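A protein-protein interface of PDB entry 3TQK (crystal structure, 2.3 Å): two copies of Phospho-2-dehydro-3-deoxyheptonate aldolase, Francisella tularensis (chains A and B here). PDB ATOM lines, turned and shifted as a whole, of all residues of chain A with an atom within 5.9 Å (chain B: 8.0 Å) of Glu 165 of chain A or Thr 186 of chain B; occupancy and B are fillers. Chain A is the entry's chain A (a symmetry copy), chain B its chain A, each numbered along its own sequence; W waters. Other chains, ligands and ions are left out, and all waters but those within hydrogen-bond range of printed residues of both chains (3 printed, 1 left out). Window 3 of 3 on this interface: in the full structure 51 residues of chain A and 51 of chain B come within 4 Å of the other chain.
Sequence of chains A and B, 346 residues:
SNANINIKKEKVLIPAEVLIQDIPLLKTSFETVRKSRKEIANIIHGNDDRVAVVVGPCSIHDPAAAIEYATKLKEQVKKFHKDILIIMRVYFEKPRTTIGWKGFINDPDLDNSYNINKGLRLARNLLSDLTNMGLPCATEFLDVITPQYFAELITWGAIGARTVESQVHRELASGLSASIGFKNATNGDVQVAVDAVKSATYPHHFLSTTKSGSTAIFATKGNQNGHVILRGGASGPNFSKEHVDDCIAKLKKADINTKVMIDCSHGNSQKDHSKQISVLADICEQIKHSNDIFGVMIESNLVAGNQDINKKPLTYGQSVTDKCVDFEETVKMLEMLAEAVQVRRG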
ATOM      1  N   ALA A 161     -13.236  11.378   0.229  1.00  0.00           N
ATOM      2  CA  ALA A 161     -13.005  12.414  -0.770  1.00  0.00           C
ATOM      3  C   ALA A 161     -13.186  11.892  -2.197  1.00  0.00           C
ATOM      4  O   ALA A 161     -13.609  12.629  -3.087  1.00  0.00           O
ATOM      5  CB  ALA A 161     -11.596  12.994  -0.610  1.00  0.00           C
ATOM      6  N   ARG A 162     -12.843  10.623  -2.401  1.00  0.00           N
ATOM      7  CA  ARG A 162     -12.861  10.023  -3.715  1.00  0.00           C
ATOM      8  C   ARG A 162     -14.256   9.615  -4.201  1.00  0.00           C
ATOM      9  O   ARG A 162     -14.424   9.349  -5.402  1.00  0.00           O
ATOM     10  CB  ARG A 162     -11.906   8.827  -3.746  1.00  0.00           C
ATOM     11  CG  ARG A 162     -10.452   9.263  -3.827  1.00  0.00           C
ATOM     12  CD  ARG A 162      -9.476   8.120  -3.818  1.00  0.00           C
ATOM     13  NE  ARG A 162      -9.798   7.080  -4.804  1.00  0.00           N
ATOM     14  CZ  ARG A 162      -8.953   6.127  -5.199  1.00  0.00           C
ATOM     15  NH1 ARG A 162      -7.711   6.082  -4.719  1.00  0.00           N
ATOM     16  NH2 ARG A 162      -9.343   5.222  -6.098  1.00  0.00           N
ATOM     17  N   THR A 163     -15.235   9.567  -3.287  1.00  0.00           N
ATOM     18  CA  THR A 163     -16.598   9.159  -3.628  1.00  0.00           C
ATOM     19  C   THR A 163     -17.651  10.243  -3.327  1.00  0.00           C
ATOM     20  O   THR A 163     -18.849   9.968  -3.370  1.00  0.00           O
ATOM     21  CB  THR A 163     -16.966   7.848  -2.921  1.00  0.00           C
ATOM     22  OG1 THR A 163     -16.573   7.918  -1.554  1.00  0.00           O
ATOM     23  CG2 THR A 163     -16.252   6.673  -3.576  1.00  0.00           C
ATOM     24  N   VAL A 164     -17.194  11.475  -3.090  1.00  0.00           N
ATOM     25  CA  VAL A 164     -18.070  12.568  -2.687  1.00  0.00           C
ATOM     26  C   VAL A 164     -19.000  13.012  -3.824  1.00  0.00           C
ATOM     27  O   VAL A 164     -20.100  13.493  -3.566  1.00  0.00           O
ATOM     28  CB  VAL A 164     -17.260  13.797  -2.153  1.00  0.00           C
ATOM     29  CG1 VAL A 164     -16.490  14.468  -3.271  1.00  0.00           C
ATOM     30  CG2 VAL A 164     -18.202  14.804  -1.472  1.00  0.00           C
ATOM     31  N   GLU A 165     -18.553  12.842  -5.068  1.00  0.00           N
ATOM     32  CA  GLU A 165     -19.387  13.100  -6.234  1.00  0.00           C
ATOM     33  C   GLU A 165     -20.140  11.854  -6.692  1.00  0.00           C
ATOM     34  O   GLU A 165     -20.810  11.884  -7.719  1.00  0.00           O
ATOM     35  CB  GLU A 165     -18.548  13.601  -7.391  1.00  0.00           C
ATOM     36  CG  GLU A 165     -18.012  15.009  -7.252  1.00  0.00           C
ATOM     37  CD  GLU A 165     -17.215  15.408  -8.474  1.00  0.00           C
ATOM     38  OE1 GLU A 165     -16.058  14.952  -8.577  1.00  0.00           O
ATOM     39  OE2 GLU A 165     -17.745  16.155  -9.326  1.00  0.00           O
ATOM     40  N   SER A 166     -20.025  10.758  -5.961  1.00  0.00           N
ATOM     41  CA  SER A 166     -20.585   9.490  -6.417  1.00  0.00           C
ATOM     42  C   SER A 166     -22.054   9.385  -6.030  1.00  0.00           C
ATOM     43  O   SER A 166     -22.402   9.451  -4.864  1.00  0.00           O
ATOM     44  CB  SER A 166     -19.817   8.327  -5.798  1.00  0.00           C
ATOM     45  OG  SER A 166     -20.413   7.093  -6.095  1.00  0.00           O
ATOM     46  N   GLN A 167     -22.900   9.183  -7.026  1.00  0.00           N
ATOM     47  CA  GLN A 167     -24.339   9.193  -6.828  1.00  0.00           C
ATOM     48  C   GLN A 167     -24.816   8.118  -5.838  1.00  0.00           C
ATOM     49  O   GLN A 167     -25.656   8.402  -4.967  1.00  0.00           O
ATOM     50  CB  GLN A 167     -25.042   9.042  -8.176  1.00  0.00           C
ATOM     51  CG  GLN A 167     -26.577   9.076  -8.112  1.00  0.00           C
ATOM     52  CD  GLN A 167     -27.146  10.346  -7.495  1.00  0.00           C
ATOM     53  OE1 GLN A 167     -28.181  10.300  -6.825  1.00  0.00           O
ATOM     54  NE2 GLN A 167     -26.483  11.476  -7.712  1.00  0.00           N
ATOM     55  N   ARG A 170     -24.127   9.134  -2.149  1.00  0.00           N
ATOM     56  CA  ARG A 170     -25.116  10.069  -1.619  1.00  0.00           C
ATOM     57  C   ARG A 170     -26.419   9.312  -1.299  1.00  0.00           C
ATOM     58  O   ARG A 170     -27.002   9.472  -0.234  1.00  0.00           O
ATOM     59  CB  ARG A 170     -25.350  11.198  -2.620  1.00  0.00           C
ATOM     60  CG  ARG A 170     -24.102  12.020  -2.902  1.00  0.00           C
ATOM     61  CD  ARG A 170     -24.214  12.836  -4.189  1.00  0.00           C
ATOM     62  NE  ARG A 170     -23.090  13.769  -4.313  1.00  0.00           N
ATOM     63  CZ  ARG A 170     -23.109  14.898  -5.011  1.00  0.00           C
ATOM     64  NH1 ARG A 170     -24.183  15.249  -5.692  1.00  0.00           N
ATOM     65  NH2 ARG A 170     -22.036  15.676  -5.047  1.00  0.00           N
ATOM     66  N   ALA A 185     -13.485  17.278  -1.986  1.00  0.00           N
ATOM     67  CA  ALA A 185     -12.841  16.531  -3.061  1.00  0.00           C
ATOM     68  C   ALA A 185     -11.312  16.522  -2.941  1.00  0.00           C
ATOM     69  O   ALA A 185     -10.724  17.403  -2.305  1.00  0.00           O
ATOM     70  CB  ALA A 185     -13.270  17.099  -4.420  1.00  0.00           C
ATOM     71  N   ASN A 187      -9.142  17.390  -4.968  1.00  0.00           N
ATOM     72  CA  ASN A 187      -8.623  18.667  -5.495  1.00  0.00           C
ATOM     73  C   ASN A 187      -8.810  19.867  -4.556  1.00  0.00           C
ATOM     74  O   ASN A 187      -8.234  20.932  -4.782  1.00  0.00           O
ATOM     75  CB  ASN A 187      -9.278  18.993  -6.845  1.00  0.00           C
ATOM     76  CG  ASN A 187     -10.786  19.100  -6.744  1.00  0.00           C
ATOM     77  OD1 ASN A 187     -11.306  19.846  -5.929  1.00  0.00           O
ATOM     78  ND2 ASN A 187     -11.491  18.300  -7.523  1.00  0.00           N
ATOM     79  N   VAL A 192     -18.734  20.487  -3.902  1.00  0.00           N
ATOM     80  CA  VAL A 192     -19.211  19.132  -4.144  1.00  0.00           C
ATOM     81  C   VAL A 192     -19.597  18.415  -2.860  1.00  0.00           C
ATOM     82  O   VAL A 192     -20.523  17.615  -2.874  1.00  0.00           O
ATOM     83  CB  VAL A 192     -18.213  18.283  -4.968  1.00  0.00           C
ATOM     84  CG1 VAL A 192     -18.039  18.910  -6.342  1.00  0.00           C
ATOM     85  CG2 VAL A 192     -16.870  18.136  -4.262  1.00  0.00           C
ATOM     86  N   ALA A 196     -23.253  17.134  -1.795  1.00  0.00           N
ATOM     87  CA  ALA A 196     -23.480  15.751  -1.411  1.00  0.00           C
ATOM     88  C   ALA A 196     -24.339  15.704  -0.159  1.00  0.00           C
ATOM     89  O   ALA A 196     -25.242  14.863  -0.044  1.00  0.00           O
ATOM     90  CB  ALA A 196     -22.160  15.015  -1.188  1.00  0.00           C
ATOM     91  N   PRO B  95     -26.451  12.381 -14.772  1.00  0.00           N
ATOM     92  CA  PRO B  95     -25.881  13.020 -13.577  1.00  0.00           C
ATOM     93  C   PRO B  95     -26.621  14.293 -13.160  1.00  0.00           C
ATOM     94  O   PRO B  95     -26.989  15.111 -14.023  1.00  0.00           O
ATOM     95  CB  PRO B  95     -24.445  13.373 -13.997  1.00  0.00           C
ATOM     96  CG  PRO B  95     -24.292  12.911 -15.458  1.00  0.00           C
ATOM     97  CD  PRO B  95     -25.418  12.001 -15.759  1.00  0.00           C
ATOM     98  N   ARG B  96     -26.815  14.453 -11.849  1.00  0.00           N
ATOM     99  CA  ARG B  96     -27.457  15.638 -11.262  1.00  0.00           C
ATOM    100  C   ARG B  96     -26.616  16.190 -10.107  1.00  0.00           C
ATOM    101  O   ARG B  96     -26.140  15.423  -9.268  1.00  0.00           O
ATOM    102  CB  ARG B  96     -28.847  15.289 -10.723  1.00  0.00           C
ATOM    103  CG  ARG B  96     -29.806  14.673 -11.741  1.00  0.00           C
ATOM    104  CD  ARG B  96     -30.266  15.682 -12.806  1.00  0.00           C
ATOM    105  NE  ARG B  96     -31.136  15.053 -13.807  1.00  0.00           N
ATOM    106  CZ  ARG B  96     -31.662  15.671 -14.865  1.00  0.00           C
ATOM    107  NH1 ARG B  96     -31.418  16.957 -15.095  1.00  0.00           N
ATOM    108  NH2 ARG B  96     -32.442  14.993 -15.703  1.00  0.00           N
ATOM    109  N   THR B  97     -26.452  17.512 -10.064  1.00  0.00           N
ATOM    110  CA  THR B  97     -25.687  18.183  -9.010  1.00  0.00           C
ATOM    111  C   THR B  97     -26.189  17.802  -7.610  1.00  0.00           C
ATOM    112  O   THR B  97     -25.386  17.523  -6.718  1.00  0.00           O
ATOM    113  CB  THR B  97     -25.757  19.718  -9.177  1.00  0.00           C
ATOM    114  OG1 THR B  97     -25.305  20.071 -10.486  1.00  0.00           O
ATOM    115  CG2 THR B  97     -24.894  20.440  -8.137  1.00  0.00           C
ATOM    116  N   GLY B 160     -17.991   7.385 -15.621  1.00  0.00           N
ATOM    117  CA  GLY B 160     -18.242   8.827 -15.704  1.00  0.00           C
ATOM    118  C   GLY B 160     -17.251   9.663 -14.929  1.00  0.00           C
ATOM    119  O   GLY B 160     -16.479   9.141 -14.123  1.00  0.00           O
ATOM    120  N   ALA B 161     -17.264  10.966 -15.184  1.00  0.00           N
ATOM    121  CA  ALA B 161     -16.353  11.901 -14.536  1.00  0.00           C
ATOM    122  C   ALA B 161     -16.488  11.878 -13.012  1.00  0.00           C
ATOM    123  O   ALA B 161     -15.513  12.093 -12.291  1.00  0.00           O
ATOM    124  CB  ALA B 161     -16.603  13.322 -15.052  1.00  0.00           C
ATOM    125  N   ARG B 162     -17.706  11.634 -12.539  1.00  0.00           N
ATOM    126  CA  ARG B 162     -18.007  11.683 -11.127  1.00  0.00           C
ATOM    127  C   ARG B 162     -17.570  10.439 -10.346  1.00  0.00           C
ATOM    128  O   ARG B 162     -17.528  10.487  -9.106  1.00  0.00           O
ATOM    129  CB  ARG B 162     -19.502  11.947 -10.929  1.00  0.00           C
ATOM    130  CG  ARG B 162     -19.862  13.402 -11.185  1.00  0.00           C
ATOM    131  CD  ARG B 162     -21.328  13.697 -11.044  1.00  0.00           C
ATOM    132  NE  ARG B 162     -21.897  13.200  -9.784  1.00  0.00           N
ATOM    133  CZ  ARG B 162     -23.074  13.578  -9.286  1.00  0.00           C
ATOM    134  NH1 ARG B 162     -23.818  14.485  -9.919  1.00  0.00           N
ATOM    135  NH2 ARG B 162     -23.507  13.063  -8.134  1.00  0.00           N
ATOM    136  N   THR B 163     -17.249   9.349 -11.057  1.00  0.00           N
ATOM    137  CA  THR B 163     -16.849   8.095 -10.420  1.00  0.00           C
ATOM    138  C   THR B 163     -15.441   7.626 -10.831  1.00  0.00           C
ATOM    139  O   THR B 163     -15.056   6.495 -10.538  1.00  0.00           O
ATOM    140  CB  THR B 163     -17.879   6.992 -10.697  1.00  0.00           C
ATOM    141  OG1 THR B 163     -18.227   7.001 -12.079  1.00  0.00           O
ATOM    142  CG2 THR B 163     -19.140   7.223  -9.875  1.00  0.00           C
ATOM    143  N   VAL B 164     -14.664   8.522 -11.448  1.00  0.00           N
ATOM    144  CA  VAL B 164     -13.353   8.180 -11.985  1.00  0.00           C
ATOM    145  C   VAL B 164     -12.332   7.894 -10.876  1.00  0.00           C
ATOM    146  O   VAL B 164     -11.403   7.118 -11.081  1.00  0.00           O
ATOM    147  CB  VAL B 164     -12.805   9.296 -12.935  1.00  0.00           C
ATOM    148  CG1 VAL B 164     -12.460  10.550 -12.161  1.00  0.00           C
ATOM    149  CG2 VAL B 164     -11.575   8.787 -13.705  1.00  0.00           C
ATOM    150  N   GLU B 165     -12.516   8.519  -9.712  1.00  0.00           N
ATOM    151  CA  GLU B 165     -11.697   8.235  -8.541  1.00  0.00           C
ATOM    152  C   GLU B 165     -12.299   7.140  -7.666  1.00  0.00           C
ATOM    153  O   GLU B 165     -11.778   6.854  -6.594  1.00  0.00           O
ATOM    154  CB  GLU B 165     -11.525   9.480  -7.695  1.00  0.00           C
ATOM    155  CG  GLU B 165     -10.626  10.549  -8.276  1.00  0.00           C
ATOM    156  CD  GLU B 165     -10.509  11.727  -7.335  1.00  0.00           C
ATOM    157  OE1 GLU B 165     -11.470  12.524  -7.292  1.00  0.00           O
ATOM    158  OE2 GLU B 165      -9.478  11.846  -6.637  1.00  0.00           O
ATOM    159  N   SER B 166     -13.397   6.540  -8.096  1.00  0.00           N
ATOM    160  CA  SER B 166     -14.118   5.597  -7.246  1.00  0.00           C
ATOM    161  C   SER B 166     -13.516   4.203  -7.365  1.00  0.00           C
ATOM    162  O   SER B 166     -13.460   3.634  -8.442  1.00  0.00           O
ATOM    163  CB  SER B 166     -15.587   5.548  -7.649  1.00  0.00           C
ATOM    164  OG  SER B 166     -16.285   4.549  -6.954  1.00  0.00           O
ATOM    165  N   LYS B 183     -13.676   8.886 -17.988  1.00  0.00           N
ATOM    166  CA  LYS B 183     -13.724  10.328 -18.171  1.00  0.00           C
ATOM    167  C   LYS B 183     -12.793  11.041 -17.194  1.00  0.00           C
ATOM    168  O   LYS B 183     -12.601  10.583 -16.071  1.00  0.00           O
ATOM    169  CB  LYS B 183     -15.166  10.820 -18.024  1.00  0.00           C
ATOM    170  CG  LYS B 183     -16.055  10.365 -19.184  1.00  0.00           C
ATOM    171  CD  LYS B 183     -17.306  11.208 -19.355  1.00  0.00           C
ATOM    172  CE  LYS B 183     -17.587  11.482 -20.834  1.00  0.00           C
ATOM    173  NZ  LYS B 183     -18.717  12.440 -21.027  1.00  0.00           N
ATOM    174  N   ASN B 184     -12.190  12.146 -17.618  1.00  0.00           N
ATOM    175  CA  ASN B 184     -11.416  12.946 -16.683  1.00  0.00           C
ATOM    176  C   ASN B 184     -12.362  13.541 -15.652  1.00  0.00           C
ATOM    177  O   ASN B 184     -13.580  13.472 -15.812  1.00  0.00           O
ATOM    178  CB  ASN B 184     -10.557  13.993 -17.386  1.00  0.00           C
ATOM    179  CG  ASN B 184     -11.357  15.106 -18.022  1.00  0.00           C
ATOM    180  OD1 ASN B 184     -11.905  15.967 -17.332  1.00  0.00           O
ATOM    181  ND2 ASN B 184     -11.372  15.134 -19.346  1.00  0.00           N
ATOM    182  N   ALA B 185     -11.804  14.063 -14.572  1.00  0.00           N
ATOM    183  CA  ALA B 185     -12.603  14.543 -13.449  1.00  0.00           C
ATOM    184  C   ALA B 185     -13.406  15.803 -13.792  1.00  0.00           C
ATOM    185  O   ALA B 185     -13.055  16.544 -14.716  1.00  0.00           O
ATOM    186  CB  ALA B 185     -11.698  14.797 -12.236  1.00  0.00           C
ATOM    187  N   THR B 186     -14.466  16.062 -13.020  1.00  0.00           N
ATOM    188  CA  THR B 186     -15.323  17.224 -13.280  1.00  0.00           C
ATOM    189  C   THR B 186     -14.537  18.541 -13.215  1.00  0.00           C
ATOM    190  O   THR B 186     -14.884  19.500 -13.898  1.00  0.00           O
ATOM    191  CB  THR B 186     -16.548  17.273 -12.336  1.00  0.00           C
ATOM    192  OG1 THR B 186     -16.119  17.411 -10.977  1.00  0.00           O
ATOM    193  CG2 THR B 186     -17.403  16.011 -12.478  1.00  0.00           C
ATOM    194  N   ASN B 187     -13.471  18.570 -12.413  1.00  0.00           N
ATOM    195  CA  ASN B 187     -12.574  19.740 -12.321  1.00  0.00           C
ATOM    196  C   ASN B 187     -11.603  19.892 -13.501  1.00  0.00           C
ATOM    197  O   ASN B 187     -10.960  20.932 -13.650  1.00  0.00           O
ATOM    198  CB  ASN B 187     -11.760  19.687 -11.019  1.00  0.00           C
ATOM    199  CG  ASN B 187     -10.917  18.433 -10.916  1.00  0.00           C
ATOM    200  OD1 ASN B 187     -10.143  18.125 -11.810  1.00  0.00           O
ATOM    201  ND2 ASN B 187     -11.117  17.668  -9.859  1.00  0.00           N
ATOM    202  N   GLY B 188     -11.468  18.842 -14.304  1.00  0.00           N
ATOM    203  CA  GLY B 188     -10.586  18.844 -15.467  1.00  0.00           C
ATOM    204  C   GLY B 188      -9.370  17.936 -15.348  1.00  0.00           C
ATOM    205  O   GLY B 188      -8.635  17.788 -16.315  1.00  0.00           O
ATOM    206  N   ASP B 189      -9.163  17.316 -14.181  1.00  0.00           N
ATOM    207  CA  ASP B 189      -7.948  16.526 -13.914  1.00  0.00           C
ATOM    208  C   ASP B 189      -7.908  15.245 -14.750  1.00  0.00           C
ATOM    209  O   ASP B 189      -8.767  14.387 -14.614  1.00  0.00           O
ATOM    210  CB  ASP B 189      -7.827  16.172 -12.417  1.00  0.00           C
ATOM    211  CG  ASP B 189      -6.422  15.699 -12.032  1.00  0.00           C
ATOM    212  OD1 ASP B 189      -5.970  14.654 -12.520  1.00  0.00           O
ATOM    213  OD2 ASP B 189      -5.753  16.381 -11.231  1.00  0.00           O
ATOM    214  N   VAL B 192      -6.122  11.600 -12.788  1.00  0.00           N
ATOM    215  CA  VAL B 192      -6.991  10.632 -12.133  1.00  0.00           C
ATOM    216  C   VAL B 192      -7.596   9.638 -13.112  1.00  0.00           C
ATOM    217  O   VAL B 192      -7.800   8.487 -12.751  1.00  0.00           O
ATOM    218  CB  VAL B 192      -8.094  11.300 -11.277  1.00  0.00           C
ATOM    219  CG1 VAL B 192      -7.445  12.095 -10.155  1.00  0.00           C
ATOM    220  CG2 VAL B 192      -9.010  12.185 -12.114  1.00  0.00           C
ATOM    221  N   ARG B 231     -13.121  15.310 -21.712  1.00  0.00           N
ATOM    222  CA  ARG B 231     -14.479  15.868 -21.728  1.00  0.00           C
ATOM    223  C   ARG B 231     -14.599  17.224 -21.040  1.00  0.00           C
ATOM    224  O   ARG B 231     -15.689  17.614 -20.635  1.00  0.00           O
ATOM    225  CB  ARG B 231     -15.472  14.876 -21.086  1.00  0.00           C
ATOM    226  CG  ARG B 231     -15.043  14.310 -19.742  1.00  0.00           C
ATOM    227  CD  ARG B 231     -15.203  15.276 -18.565  1.00  0.00           C
ATOM    228  NE  ARG B 231     -16.608  15.539 -18.250  1.00  0.00           N
ATOM    229  CZ  ARG B 231     -17.046  16.541 -17.492  1.00  0.00           C
ATOM    230  NH1 ARG B 231     -16.207  17.417 -16.956  1.00  0.00           N
ATOM    231  NH2 ARG B 231     -18.348  16.666 -17.269  1.00  0.00           N
ATOM    232  N   GLY B 232     -13.491  17.935 -20.911  1.00  0.00           N
ATOM    233  CA  GLY B 232     -13.500  19.249 -20.281  1.00  0.00           C
ATOM    234  C   GLY B 232     -13.697  19.213 -18.778  1.00  0.00           C
ATOM    235  O   GLY B 232     -13.473  18.187 -18.133  1.00  0.00           O
ATOM    236  N   GLY B 233     -14.119  20.345 -18.223  1.00  0.00           N
ATOM    237  CA  GLY B 233     -14.295  20.491 -16.773  1.00  0.00           C
ATOM    238  C   GLY B 233     -13.973  21.906 -16.339  1.00  0.00           C
ATOM    239  O   GLY B 233     -13.783  22.772 -17.180  1.00  0.00           O
ATOM    240  N   ALA B 234     -13.892  22.140 -15.030  1.00  0.00           N
ATOM    241  CA  ALA B 234     -13.672  23.494 -14.487  1.00  0.00           C
ATOM    242  C   ALA B 234     -12.391  24.152 -15.011  1.00  0.00           C
ATOM    243  O   ALA B 234     -12.337  25.371 -15.132  1.00  0.00           O
ATOM    244  CB  ALA B 234     -13.667  23.464 -12.964  1.00  0.00           C
ATOM    245  N   SER B 235     -11.377  23.339 -15.318  1.00  0.00           N
ATOM    246  CA  SER B 235     -10.130  23.797 -15.971  1.00  0.00           C
ATOM    247  C   SER B 235     -10.344  24.390 -17.368  1.00  0.00           C
ATOM    248  O   SER B 235      -9.446  25.029 -17.921  1.00  0.00           O
ATOM    249  CB  SER B 235      -9.177  22.605 -16.156  1.00  0.00           C
ATOM    250  OG  SER B 235      -8.570  22.204 -14.957  1.00  0.00           O
ATOM    251  N   GLY B 236     -11.502  24.113 -17.961  1.00  0.00           N
ATOM    252  CA  GLY B 236     -11.807  24.513 -19.332  1.00  0.00           C
ATOM    253  C   GLY B 236     -11.688  23.336 -20.292  1.00  0.00           C
ATOM    254  O   GLY B 236     -11.253  22.256 -19.905  1.00  0.00           O
ATOM    255  N   GLY B 267     -18.426  19.173 -21.112  1.00  0.00           N
ATOM    256  CA  GLY B 267     -17.478  20.237 -20.780  1.00  0.00           C
ATOM    257  C   GLY B 267     -16.728  20.840 -21.958  1.00  0.00           C
ATOM    258  O   GLY B 267     -16.300  21.999 -21.894  1.00  0.00           O
HETATM  259  O   HOH W   1     -14.621  14.110 -10.690  1.00  0.00           O
HETATM  260  O   HOH W   2     -22.037  17.905  -6.890  1.00  0.00           O
HETATM  261  O   HOH W   3     -12.596  13.901  -5.275  1.00  0.00           O
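Printed residues of chain B within 4 Å of Arg 162 of chain A: Glu 165 (2.7 Å). Of chain B, only Arg 162 (2.7 Å) and Thr 186 (2.6 Å) come within 4 Å of Glu 165 of chain A. Pro 95 of chain B touches none of the printed residues of chain A. Of the printed residues of chain A, Thr 97 of chain B touches Arg 170 (2.8 Å). Thr 186 of chain B touches just one residue of chain A: Glu 165. The nearest residue of chain B that does not touch Glu 165 of chain A is Ala 161 of chain B (4.7 Å).
The backbone carbonyl oxygen (O) of Thr 97 of chain B sits at hydrogen-bond distance from the guanidinium group (NH1) of Arg 170 of chain A (2.8 Å). O of Glu 165 of chain A lies within hydrogen-bond range of NE of Arg 162 of chain B (2.7 Å). NH2 of Arg 162 of chain B sits close to NE2 of Gln 167 of chain A. The guanidinium group (NE) of Arg 162 of chain A sits at hydrogen-bond distance from the backbone carbonyl oxygen (O) of Glu 165 of chain B (2.7 Å). OG1 of Thr 186 of chain B sits at hydrogen-bond distance from OE2 of Glu 165 of chain A, at 2.6 Å. The side-chain amide nitrogen of Asn 187 of chain B lies close to the side-chain amide nitrogen of Asn 187 of chain A (2.4 Å). NH2 of Arg 162 of chain B sits close to NH1 of Arg 170 of chain A (3.3 Å).
Thr 163 of chain A touches Ser 166 of chain B (CG2 to OG, 3.99 Å). Ser 166 of chain A touches Thr 163 of chain B.
Water W3 bridges OE1 of Glu 165 of chain B and O of Ala 161 of chain A. Water W1 lies within hydrogen-bond range of the side-chain carboxylate (OE1) of Glu 165 of chain A, the backbone carbonyl oxygen (O) of Ala 161 of chain B and the backbone NH (N) of Thr 186 of chain B. Water W2 bridges NH2 of Arg 170 of chain A (2.9 Å) and O of Thr 97 of chain B (3.4 Å).
The backbone carbonyl oxygen (O) of Gly 160 of chain B sits at hydrogen-bond distance from the side-chain hydroxyl (OG1) of Thr 163 of chain B, at 3.4 Å. The backbone carbonyl oxygen of Thr 186 of chain B is in hydrogen-bond range of the backbone NH of Ala 234 of chain B (3.0 Å). The side-chain amide oxygen (OD1) of Asn 187 of chain B lies within hydrogen-bond range of the backbone NH (N) of Asp 189 of chain B. The backbone carbonyl oxygen of Asn 187 of chain B sits at hydrogen-bond distance from the backbone NH of Ser 235 of chain B, at 3.0 Å. The backbone carbonyl oxygen (O) of Val 164 of chain A sits at hydrogen-bond distance from the guanidinium group (NE) of Arg 170 of chain A (3.1 Å). NH2 of Arg 170 of chain A sits at hydrogen-bond distance from O of Val 192 of chain A, at 3.3 Å.
Of the 12 printed residues of chain A, 7 touch a printed residue of chain B.
Arg 162 of chain A touches Glu 165 of chain B, and with the chains exchanged Glu 165 of chain A touches Arg 162 of chain B. Thr 163 of chain A touches Ser 166 of chain B, and with the chains exchanged Ser 166 of chain A touches Thr 163 of chain B. Asn 187 of chain B touches its own counterpart, Asn 187 of chain A. 9 positions are printed for both chains. Of the 9 pairs that touch across the chains among the printed residues, 5 have their exchanged pair printed and touching as well.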
